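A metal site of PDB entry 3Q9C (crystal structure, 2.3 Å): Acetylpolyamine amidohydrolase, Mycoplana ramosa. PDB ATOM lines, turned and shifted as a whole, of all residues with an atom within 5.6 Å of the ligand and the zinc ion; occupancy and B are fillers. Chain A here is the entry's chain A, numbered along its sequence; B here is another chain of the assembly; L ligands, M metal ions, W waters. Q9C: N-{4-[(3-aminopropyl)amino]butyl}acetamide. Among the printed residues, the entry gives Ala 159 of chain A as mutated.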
ATOM      1  N   GLU A  17      24.621  22.550  25.307  1.00  0.00           N
ATOM      2  CA  GLU A  17      23.808  21.507  25.876  1.00  0.00           C
ATOM      3  C   GLU A  17      24.561  21.073  27.122  1.00  0.00           C
ATOM      4  O   GLU A  17      25.776  20.858  27.058  1.00  0.00           O
ATOM      5  CB  GLU A  17      23.665  20.304  24.944  1.00  0.00           C
ATOM      6  CG  GLU A  17      22.581  19.352  25.410  1.00  0.00           C
ATOM      7  CD  GLU A  17      22.530  18.036  24.662  1.00  0.00           C
ATOM      8  OE1 GLU A  17      22.490  18.048  23.418  1.00  0.00           O
ATOM      9  OE2 GLU A  17      22.508  16.967  25.336  1.00  0.00           O
ATOM     10  N   TYR A  19      25.746  18.488  29.449  1.00  0.00           N
ATOM     11  CA  TYR A  19      25.927  17.045  29.418  1.00  0.00           C
ATOM     12  C   TYR A  19      27.237  16.602  30.070  1.00  0.00           C
ATOM     13  O   TYR A  19      28.314  17.108  29.723  1.00  0.00           O
ATOM     14  CB  TYR A  19      25.901  16.548  27.972  1.00  0.00           C
ATOM     15  CG  TYR A  19      26.324  15.106  27.804  1.00  0.00           C
ATOM     16  CD1 TYR A  19      25.589  14.068  28.368  1.00  0.00           C
ATOM     17  CD2 TYR A  19      27.455  14.786  27.060  1.00  0.00           C
ATOM     18  CE1 TYR A  19      25.966  12.735  28.193  1.00  0.00           C
ATOM     19  CE2 TYR A  19      27.845  13.456  26.875  1.00  0.00           C
ATOM     20  CZ  TYR A  19      27.100  12.436  27.452  1.00  0.00           C
ATOM     21  OH  TYR A  19      27.479  11.128  27.249  1.00  0.00           O
ATOM     22  N   GLU A 117      19.175  19.821  30.474  1.00  0.00           N
ATOM     23  CA  GLU A 117      20.052  19.480  29.353  1.00  0.00           C
ATOM     24  C   GLU A 117      19.566  20.107  28.037  1.00  0.00           C
ATOM     25  O   GLU A 117      20.065  19.767  26.963  1.00  0.00           O
ATOM     26  CB  GLU A 117      20.138  17.961  29.211  1.00  0.00           C
ATOM     27  CG  GLU A 117      18.820  17.206  29.380  1.00  0.00           C
ATOM     28  CD  GLU A 117      17.810  17.511  28.301  1.00  0.00           C
ATOM     29  OE1 GLU A 117      17.000  18.454  28.468  1.00  0.00           O
ATOM     30  OE2 GLU A 117      17.818  16.809  27.276  1.00  0.00           O
ATOM     31  N   PRO A 156      12.407  18.210  17.603  1.00  0.00           N
ATOM     32  CA  PRO A 156      11.447  17.138  17.888  1.00  0.00           C
ATOM     33  C   PRO A 156      10.511  17.622  18.996  1.00  0.00           C
ATOM     34  O   PRO A 156      10.662  18.754  19.467  1.00  0.00           O
ATOM     35  CB  PRO A 156      12.351  15.998  18.350  1.00  0.00           C
ATOM     36  CG  PRO A 156      13.413  16.737  19.103  1.00  0.00           C
ATOM     37  CD  PRO A 156      13.718  17.930  18.211  1.00  0.00           C
ATOM     38  N   GLY A 157       9.546  16.796  19.406  1.00  0.00           N
ATOM     39  CA  GLY A 157       8.631  17.255  20.439  1.00  0.00           C
ATOM     40  C   GLY A 157       8.162  16.285  21.496  1.00  0.00           C
ATOM     41  O   GLY A 157       7.624  16.717  22.521  1.00  0.00           O
ATOM     42  N   HIS A 158       8.375  14.987  21.295  1.00  0.00           N
ATOM     43  CA  HIS A 158       7.841  14.031  22.257  1.00  0.00           C
ATOM     44  C   HIS A 158       8.187  14.205  23.750  1.00  0.00           C
ATOM     45  O   HIS A 158       7.484  13.638  24.600  1.00  0.00           O
ATOM     46  CB  HIS A 158       8.119  12.598  21.797  1.00  0.00           C
ATOM     47  CG  HIS A 158       9.487  12.091  22.127  1.00  0.00           C
ATOM     48  ND1 HIS A 158       9.763  10.746  22.180  1.00  0.00           N
ATOM     49  CD2 HIS A 158      10.648  12.728  22.421  1.00  0.00           C
ATOM     50  CE1 HIS A 158      11.035  10.571  22.498  1.00  0.00           C
ATOM     51  NE2 HIS A 158      11.591  11.757  22.645  1.00  0.00           N
ATOM     52  N   ALA A 159       9.222  14.970  24.085  1.00  0.00           N
ATOM     53  CA  ALA A 159       9.565  15.174  25.491  1.00  0.00           C
ATOM     54  C   ALA A 159       8.872  16.422  26.072  1.00  0.00           C
ATOM     55  O   ALA A 159       8.953  16.679  27.280  1.00  0.00           O
ATOM     56  CB  ALA A 159      11.102  15.270  25.676  1.00  0.00           C
ATOM     57  N   GLY A 167      14.414  17.701  26.922  1.00  0.00           N
ATOM     58  CA  GLY A 167      14.754  16.654  25.971  1.00  0.00           C
ATOM     59  C   GLY A 167      14.833  17.157  24.544  1.00  0.00           C
ATOM     60  O   GLY A 167      14.526  16.434  23.599  1.00  0.00           O
ATOM     61  N   TYR A 168      15.270  18.406  24.403  1.00  0.00           N
ATOM     62  CA  TYR A 168      15.411  19.069  23.118  1.00  0.00           C
ATOM     63  C   TYR A 168      14.052  19.373  22.486  1.00  0.00           C
ATOM     64  O   TYR A 168      13.980  19.691  21.293  1.00  0.00           O
ATOM     65  CB  TYR A 168      16.227  18.221  22.144  1.00  0.00           C
ATOM     66  CG  TYR A 168      17.397  17.463  22.715  1.00  0.00           C
ATOM     67  CD1 TYR A 168      18.158  17.986  23.771  1.00  0.00           C
ATOM     68  CD2 TYR A 168      17.785  16.252  22.159  1.00  0.00           C
ATOM     69  CE1 TYR A 168      19.276  17.309  24.253  1.00  0.00           C
ATOM     70  CE2 TYR A 168      18.909  15.570  22.630  1.00  0.00           C
ATOM     71  CZ  TYR A 168      19.639  16.104  23.668  1.00  0.00           C
ATOM     72  OH  TYR A 168      20.754  15.430  24.120  1.00  0.00           O
ATOM     73  N   CYS A 169      12.981  19.288  23.266  1.00  0.00           N
ATOM     74  CA  CYS A 169      11.645  19.521  22.726  1.00  0.00           C
ATOM     75  C   CYS A 169      10.915  20.706  23.365  1.00  0.00           C
ATOM     76  O   CYS A 169      11.090  20.994  24.558  1.00  0.00           O
ATOM     77  CB  CYS A 169      10.789  18.255  22.895  1.00  0.00           C
ATOM     78  SG  CYS A 169      11.644  16.709  22.435  1.00  0.00           S
ATOM     79  N   ASP A 195      10.834   5.989  19.441  1.00  0.00           N
ATOM     80  CA  ASP A 195      12.063   6.700  19.757  1.00  0.00           C
ATOM     81  C   ASP A 195      12.643   5.948  20.964  1.00  0.00           C
ATOM     82  O   ASP A 195      11.888   5.421  21.771  1.00  0.00           O
ATOM     83  CB  ASP A 195      11.735   8.150  20.121  1.00  0.00           C
ATOM     84  CG  ASP A 195      12.939   8.923  20.556  1.00  0.00           C
ATOM     85  OD1 ASP A 195      13.525   8.570  21.610  1.00  0.00           O
ATOM     86  OD2 ASP A 195      13.320   9.880  19.837  1.00  0.00           O
ATOM     87  N   PHE A 196      13.965   5.882  21.078  1.00  0.00           N
ATOM     88  CA  PHE A 196      14.594   5.147  22.192  1.00  0.00           C
ATOM     89  C   PHE A 196      14.116   5.632  23.561  1.00  0.00           C
ATOM     90  O   PHE A 196      13.926   4.836  24.464  1.00  0.00           O
ATOM     91  CB  PHE A 196      16.127   5.270  22.119  1.00  0.00           C
ATOM     92  CG  PHE A 196      16.827   4.703  23.325  1.00  0.00           C
ATOM     93  CD1 PHE A 196      16.992   3.324  23.472  1.00  0.00           C
ATOM     94  CD2 PHE A 196      17.283   5.550  24.332  1.00  0.00           C
ATOM     95  CE1 PHE A 196      17.599   2.790  24.627  1.00  0.00           C
ATOM     96  CE2 PHE A 196      17.893   5.039  25.489  1.00  0.00           C
ATOM     97  CZ  PHE A 196      18.052   3.652  25.636  1.00  0.00           C
ATOM     98  N   HIS A 197      13.949   6.938  23.689  1.00  0.00           N
ATOM     99  CA  HIS A 197      13.517   7.542  24.945  1.00  0.00           C
ATOM    100  C   HIS A 197      12.009   7.510  25.076  1.00  0.00           C
ATOM    101  O   HIS A 197      11.285   7.576  24.085  1.00  0.00           O
ATOM    102  CB  HIS A 197      13.983   8.995  25.013  1.00  0.00           C
ATOM    103  CG  HIS A 197      15.466   9.143  24.905  1.00  0.00           C
ATOM    104  ND1 HIS A 197      16.089   9.729  23.831  1.00  0.00           N
ATOM    105  CD2 HIS A 197      16.450   8.745  25.745  1.00  0.00           C
ATOM    106  CE1 HIS A 197      17.397   9.683  24.008  1.00  0.00           C
ATOM    107  NE2 HIS A 197      17.648   9.087  25.162  1.00  0.00           N
ATOM    108  N   PHE A 225      17.176   8.452  30.269  1.00  0.00           N
ATOM    109  CA  PHE A 225      16.387   9.676  30.190  1.00  0.00           C
ATOM    110  C   PHE A 225      15.012   9.257  29.630  1.00  0.00           C
ATOM    111  O   PHE A 225      14.949   8.415  28.737  1.00  0.00           O
ATOM    112  CB  PHE A 225      17.075  10.656  29.230  1.00  0.00           C
ATOM    113  CG  PHE A 225      16.523  12.049  29.261  1.00  0.00           C
ATOM    114  CD1 PHE A 225      17.028  12.990  30.143  1.00  0.00           C
ATOM    115  CD2 PHE A 225      15.480  12.404  28.401  1.00  0.00           C
ATOM    116  CE1 PHE A 225      16.506  14.287  30.174  1.00  0.00           C
ATOM    117  CE2 PHE A 225      14.952  13.694  28.431  1.00  0.00           C
ATOM    118  CZ  PHE A 225      15.457  14.634  29.313  1.00  0.00           C
ATOM    119  N   ASP A 284      17.066   6.497  17.208  1.00  0.00           N
ATOM    120  CA  ASP A 284      18.147   6.419  18.153  1.00  0.00           C
ATOM    121  C   ASP A 284      18.237   5.069  18.862  1.00  0.00           C
ATOM    122  O   ASP A 284      19.026   4.884  19.777  1.00  0.00           O
ATOM    123  CB  ASP A 284      18.106   7.592  19.165  1.00  0.00           C
ATOM    124  CG  ASP A 284      16.718   7.887  19.712  1.00  0.00           C
ATOM    125  OD1 ASP A 284      15.706   7.361  19.198  1.00  0.00           O
ATOM    126  OD2 ASP A 284      16.642   8.678  20.680  1.00  0.00           O
ATOM    127  N   ILE A 291      24.102   7.875  22.576  1.00  0.00           N
ATOM    128  CA  ILE A 291      23.360   8.000  23.827  1.00  0.00           C
ATOM    129  C   ILE A 291      22.218   7.004  24.021  1.00  0.00           C
ATOM    130  O   ILE A 291      21.199   7.337  24.607  1.00  0.00           O
ATOM    131  CB  ILE A 291      22.759   9.435  24.007  1.00  0.00           C
ATOM    132  CG1 ILE A 291      21.793   9.748  22.845  1.00  0.00           C
ATOM    133  CG2 ILE A 291      23.874  10.462  24.090  1.00  0.00           C
ATOM    134  CD1 ILE A 291      20.989  11.058  23.017  1.00  0.00           C
ATOM    135  N   GLU A 320      11.596  12.414  15.317  1.00  0.00           N
ATOM    136  CA  GLU A 320      11.943  12.728  16.713  1.00  0.00           C
ATOM    137  C   GLU A 320      13.469  12.621  16.899  1.00  0.00           C
ATOM    138  O   GLU A 320      14.212  13.360  16.255  1.00  0.00           O
ATOM    139  CB  GLU A 320      11.231  11.765  17.686  1.00  0.00           C
ATOM    140  CG  GLU A 320       9.707  11.767  17.620  1.00  0.00           C
ATOM    141  CD  GLU A 320       9.047  12.919  18.401  1.00  0.00           C
ATOM    142  OE1 GLU A 320       9.775  13.815  18.880  1.00  0.00           O
ATOM    143  OE2 GLU A 320       7.798  12.921  18.517  1.00  0.00           O
ATOM    144  N   GLY A 321      13.922  11.693  17.755  1.00  0.00           N
ATOM    145  CA  GLY A 321      15.353  11.527  18.013  1.00  0.00           C
ATOM    146  C   GLY A 321      16.157  10.740  16.985  1.00  0.00           C
ATOM    147  O   GLY A 321      15.643  10.296  15.961  1.00  0.00           O
ATOM    148  N   GLY A 322      17.446  10.541  17.290  1.00  0.00           N
ATOM    149  CA  GLY A 322      18.344   9.827  16.384  1.00  0.00           C
ATOM    150  C   GLY A 322      19.527  10.766  16.252  1.00  0.00           C
ATOM    151  O   GLY A 322      19.380  11.876  15.755  1.00  0.00           O
ATOM    152  N   TYR A 323      20.717  10.324  16.661  1.00  0.00           N
ATOM    153  CA  TYR A 323      21.856  11.216  16.628  1.00  0.00           C
ATOM    154  C   TYR A 323      23.154  10.677  16.084  1.00  0.00           C
ATOM    155  O   TYR A 323      23.225   9.545  15.607  1.00  0.00           O
ATOM    156  CB  TYR A 323      22.097  11.743  18.032  1.00  0.00           C
ATOM    157  CG  TYR A 323      20.813  12.116  18.741  1.00  0.00           C
ATOM    158  CD1 TYR A 323      20.250  13.377  18.579  1.00  0.00           C
ATOM    159  CD2 TYR A 323      20.139  11.172  19.522  1.00  0.00           C
ATOM    160  CE1 TYR A 323      19.039  13.701  19.177  1.00  0.00           C
ATOM    161  CE2 TYR A 323      18.916  11.480  20.119  1.00  0.00           C
ATOM    162  CZ  TYR A 323      18.380  12.747  19.936  1.00  0.00           C
ATOM    163  OH  TYR A 323      17.191  13.068  20.523  1.00  0.00           O
ATOM    164  N   TYR B  83      31.966  10.449  32.685  1.00  0.00           N
ATOM    165  CA  TYR B  83      31.719  11.878  32.487  1.00  0.00           C
ATOM    166  C   TYR B  83      32.946  12.728  32.777  1.00  0.00           C
ATOM    167  O   TYR B  83      33.700  12.456  33.716  1.00  0.00           O
ATOM    168  CB  TYR B  83      30.524  12.315  33.327  1.00  0.00           C
ATOM    169  CG  TYR B  83      29.259  11.612  32.893  1.00  0.00           C
ATOM    170  CD1 TYR B  83      28.844  11.654  31.566  1.00  0.00           C
ATOM    171  CD2 TYR B  83      28.517  10.860  33.798  1.00  0.00           C
ATOM    172  CE1 TYR B  83      27.713  10.964  31.134  1.00  0.00           C
ATOM    173  CE2 TYR B  83      27.389  10.154  33.385  1.00  0.00           C
ATOM    174  CZ  TYR B  83      26.986  10.213  32.049  1.00  0.00           C
ATOM    175  OH  TYR B  83      25.877   9.518  31.625  1.00  0.00           O
ATOM    176  N   THR B  90      20.517  16.782  35.314  1.00  0.00           N
ATOM    177  CA  THR B  90      19.922  17.323  34.108  1.00  0.00           C
ATOM    178  C   THR B  90      18.442  16.996  34.018  1.00  0.00           C
ATOM    179  O   THR B  90      17.642  17.800  33.546  1.00  0.00           O
ATOM    180  CB  THR B  90      20.645  16.779  32.848  1.00  0.00           C
ATOM    181  OG1 THR B  90      20.791  15.366  32.953  1.00  0.00           O
ATOM    182  CG2 THR B  90      22.002  17.430  32.696  1.00  0.00           C
ATOM    183  N   GLU B 106      23.154   8.799  36.607  1.00  0.00           N
ATOM    184  CA  GLU B 106      22.560   9.956  35.964  1.00  0.00           C
ATOM    185  C   GLU B 106      21.105  10.182  36.388  1.00  0.00           C
ATOM    186  O   GLU B 106      20.644  11.322  36.430  1.00  0.00           O
ATOM    187  CB  GLU B 106      22.665   9.826  34.444  1.00  0.00           C
ATOM    188  CG  GLU B 106      22.889  11.145  33.740  1.00  0.00           C
ATOM    189  CD  GLU B 106      23.016  11.010  32.228  1.00  0.00           C
ATOM    190  OE1 GLU B 106      23.296  12.039  31.563  1.00  0.00           O
ATOM    191  OE2 GLU B 106      22.842   9.872  31.717  1.00  0.00           O
HETATM  192  N   Q9C L   1      23.275  10.828  29.141  1.00  0.00           N
HETATM  193  C   Q9C L   1      14.758  13.291  21.981  1.00  0.00           C
HETATM  194  O   Q9C L   1      14.944  12.134  21.564  1.00  0.00           O
HETATM  195  N01 Q9C L   1      19.707  13.663  27.405  1.00  0.00           N
HETATM  196  N02 Q9C L   1      15.572  13.730  22.954  1.00  0.00           N
HETATM  197  C01 Q9C L   1      21.094  13.255  27.170  1.00  0.00           C
HETATM  198  C02 Q9C L   1      22.367  11.207  28.052  1.00  0.00           C
HETATM  199  C03 Q9C L   1      18.726  12.931  26.567  1.00  0.00           C
HETATM  200  C04 Q9C L   1      16.628  13.099  23.646  1.00  0.00           C
HETATM  201  C05 Q9C L   1      21.630  12.522  28.411  1.00  0.00           C
HETATM  202  C06 Q9C L   1      18.036  13.925  25.633  1.00  0.00           C
HETATM  203  C07 Q9C L   1      16.645  13.489  25.142  1.00  0.00           C
HETATM  204  C08 Q9C L   1      13.693  14.037  21.331  1.00  0.00           C
HETATM  205 ZN    ZN M   1      15.381  10.052  21.615  1.00  0.00          ZN
HETATM  206  O   HOH W   1      20.134   9.479  26.438  1.00  0.00           O
HETATM  207  O   HOH W   2      13.746  12.635  24.817  1.00  0.00           O
HETATM  208  O   HOH W   3      22.511  16.070  28.331  1.00  0.00           O
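OE1 of Glu 106 of chain B lies within salt-bridge range of N of the ligand, 2.7 Å away. A nitrogen (N02) of the ligand sits at hydrogen-bond distance from the backbone carbonyl oxygen of Gly 167, 3.0 Å away. A nitrogen (N01) of the ligand is in salt-bridge range of the side-chain carboxylate (OE2) of Glu 117 (3.7 Å). OH of Tyr 323 sits close to N02 of the ligand, 3.0 Å away.
OE1 of Glu 117 is in hydrogen-bond range of N of Gly 167 (3.1 Å). The backbone NH (N) of Ala 159 lies within hydrogen-bond range of the side-chain sulfur (SG) of Cys 169, 3.4 Å away. OD1 of Asp 284 lies within hydrogen-bond range of N of Phe 196 (3.0 Å). SG of Cys 169 lies close to N of Gly 157, at 3.7 Å. The backbone carbonyl oxygen (O) of Pro 156 lies close to the side-chain sulfur (SG) of Cys 169 (3.7 Å). O of Gly 167 sits at hydrogen-bond distance from SG of Cys 169 (3.1 Å). The side-chain carboxylate (OE1) of Glu 320 lies within hydrogen-bond range of the backbone NH (N) of His 158 (3.0 Å). OE2 of Glu 106 of chain B lies within hydrogen-bond range of OH of Tyr 83 of chain B (3.1 Å).
Residues that only touch the ligand: Tyr 168 (3.3 Å), His 158 (3.4 Å), Tyr 19 (3.4 Å), Pro 156 (3.5 Å), Cys 169 (3.5 Å), Phe 225 (3.6 Å), Gly 321 (3.6 Å) and Tyr 83 of chain B (3.8 Å). Hydrophobic or aromatic side chains that line the ligand: Tyr 19, Pro 156, His 158, Tyr 168, His 197, Phe 225 and Tyr 323. The nearest printed residue that does not touch the ligand is Ile 291 (4.3 Å).
Merely in contact with the zinc ion: Gly 321 and Tyr 323. Of the 23 residues printed, 5 come within 4 Å of the zinc ion. Along chain A the residues within 4 Å of the zinc ion span positions 195 to 323. The nearest printed residue that does not touch the zinc ion is His 158 (4.3 Å).
The zinc ion is bound by the side-chain carboxylate (OD2) of Asp 284 (2.1 Å). O of the ligand is bound to the zinc ion. A ring nitrogen (ND1) of His 197 binds the zinc ion, 2.3 Å away. The zinc ion is bound by OD1 of Asp 195, at 2.4 Å. Slightly farther from the zinc ion lies OD2 of Asp 195 (2.7 Å).
Water W2 lies within hydrogen-bond range of N02 of the ligand (2.8 Å) and NE2 of His 158 (3.2 Å). Water W1 bridges a ring nitrogen (NE2) of His 197 (2.8 Å) and the backbone carbonyl oxygen of Ile 291 (3.0 Å).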
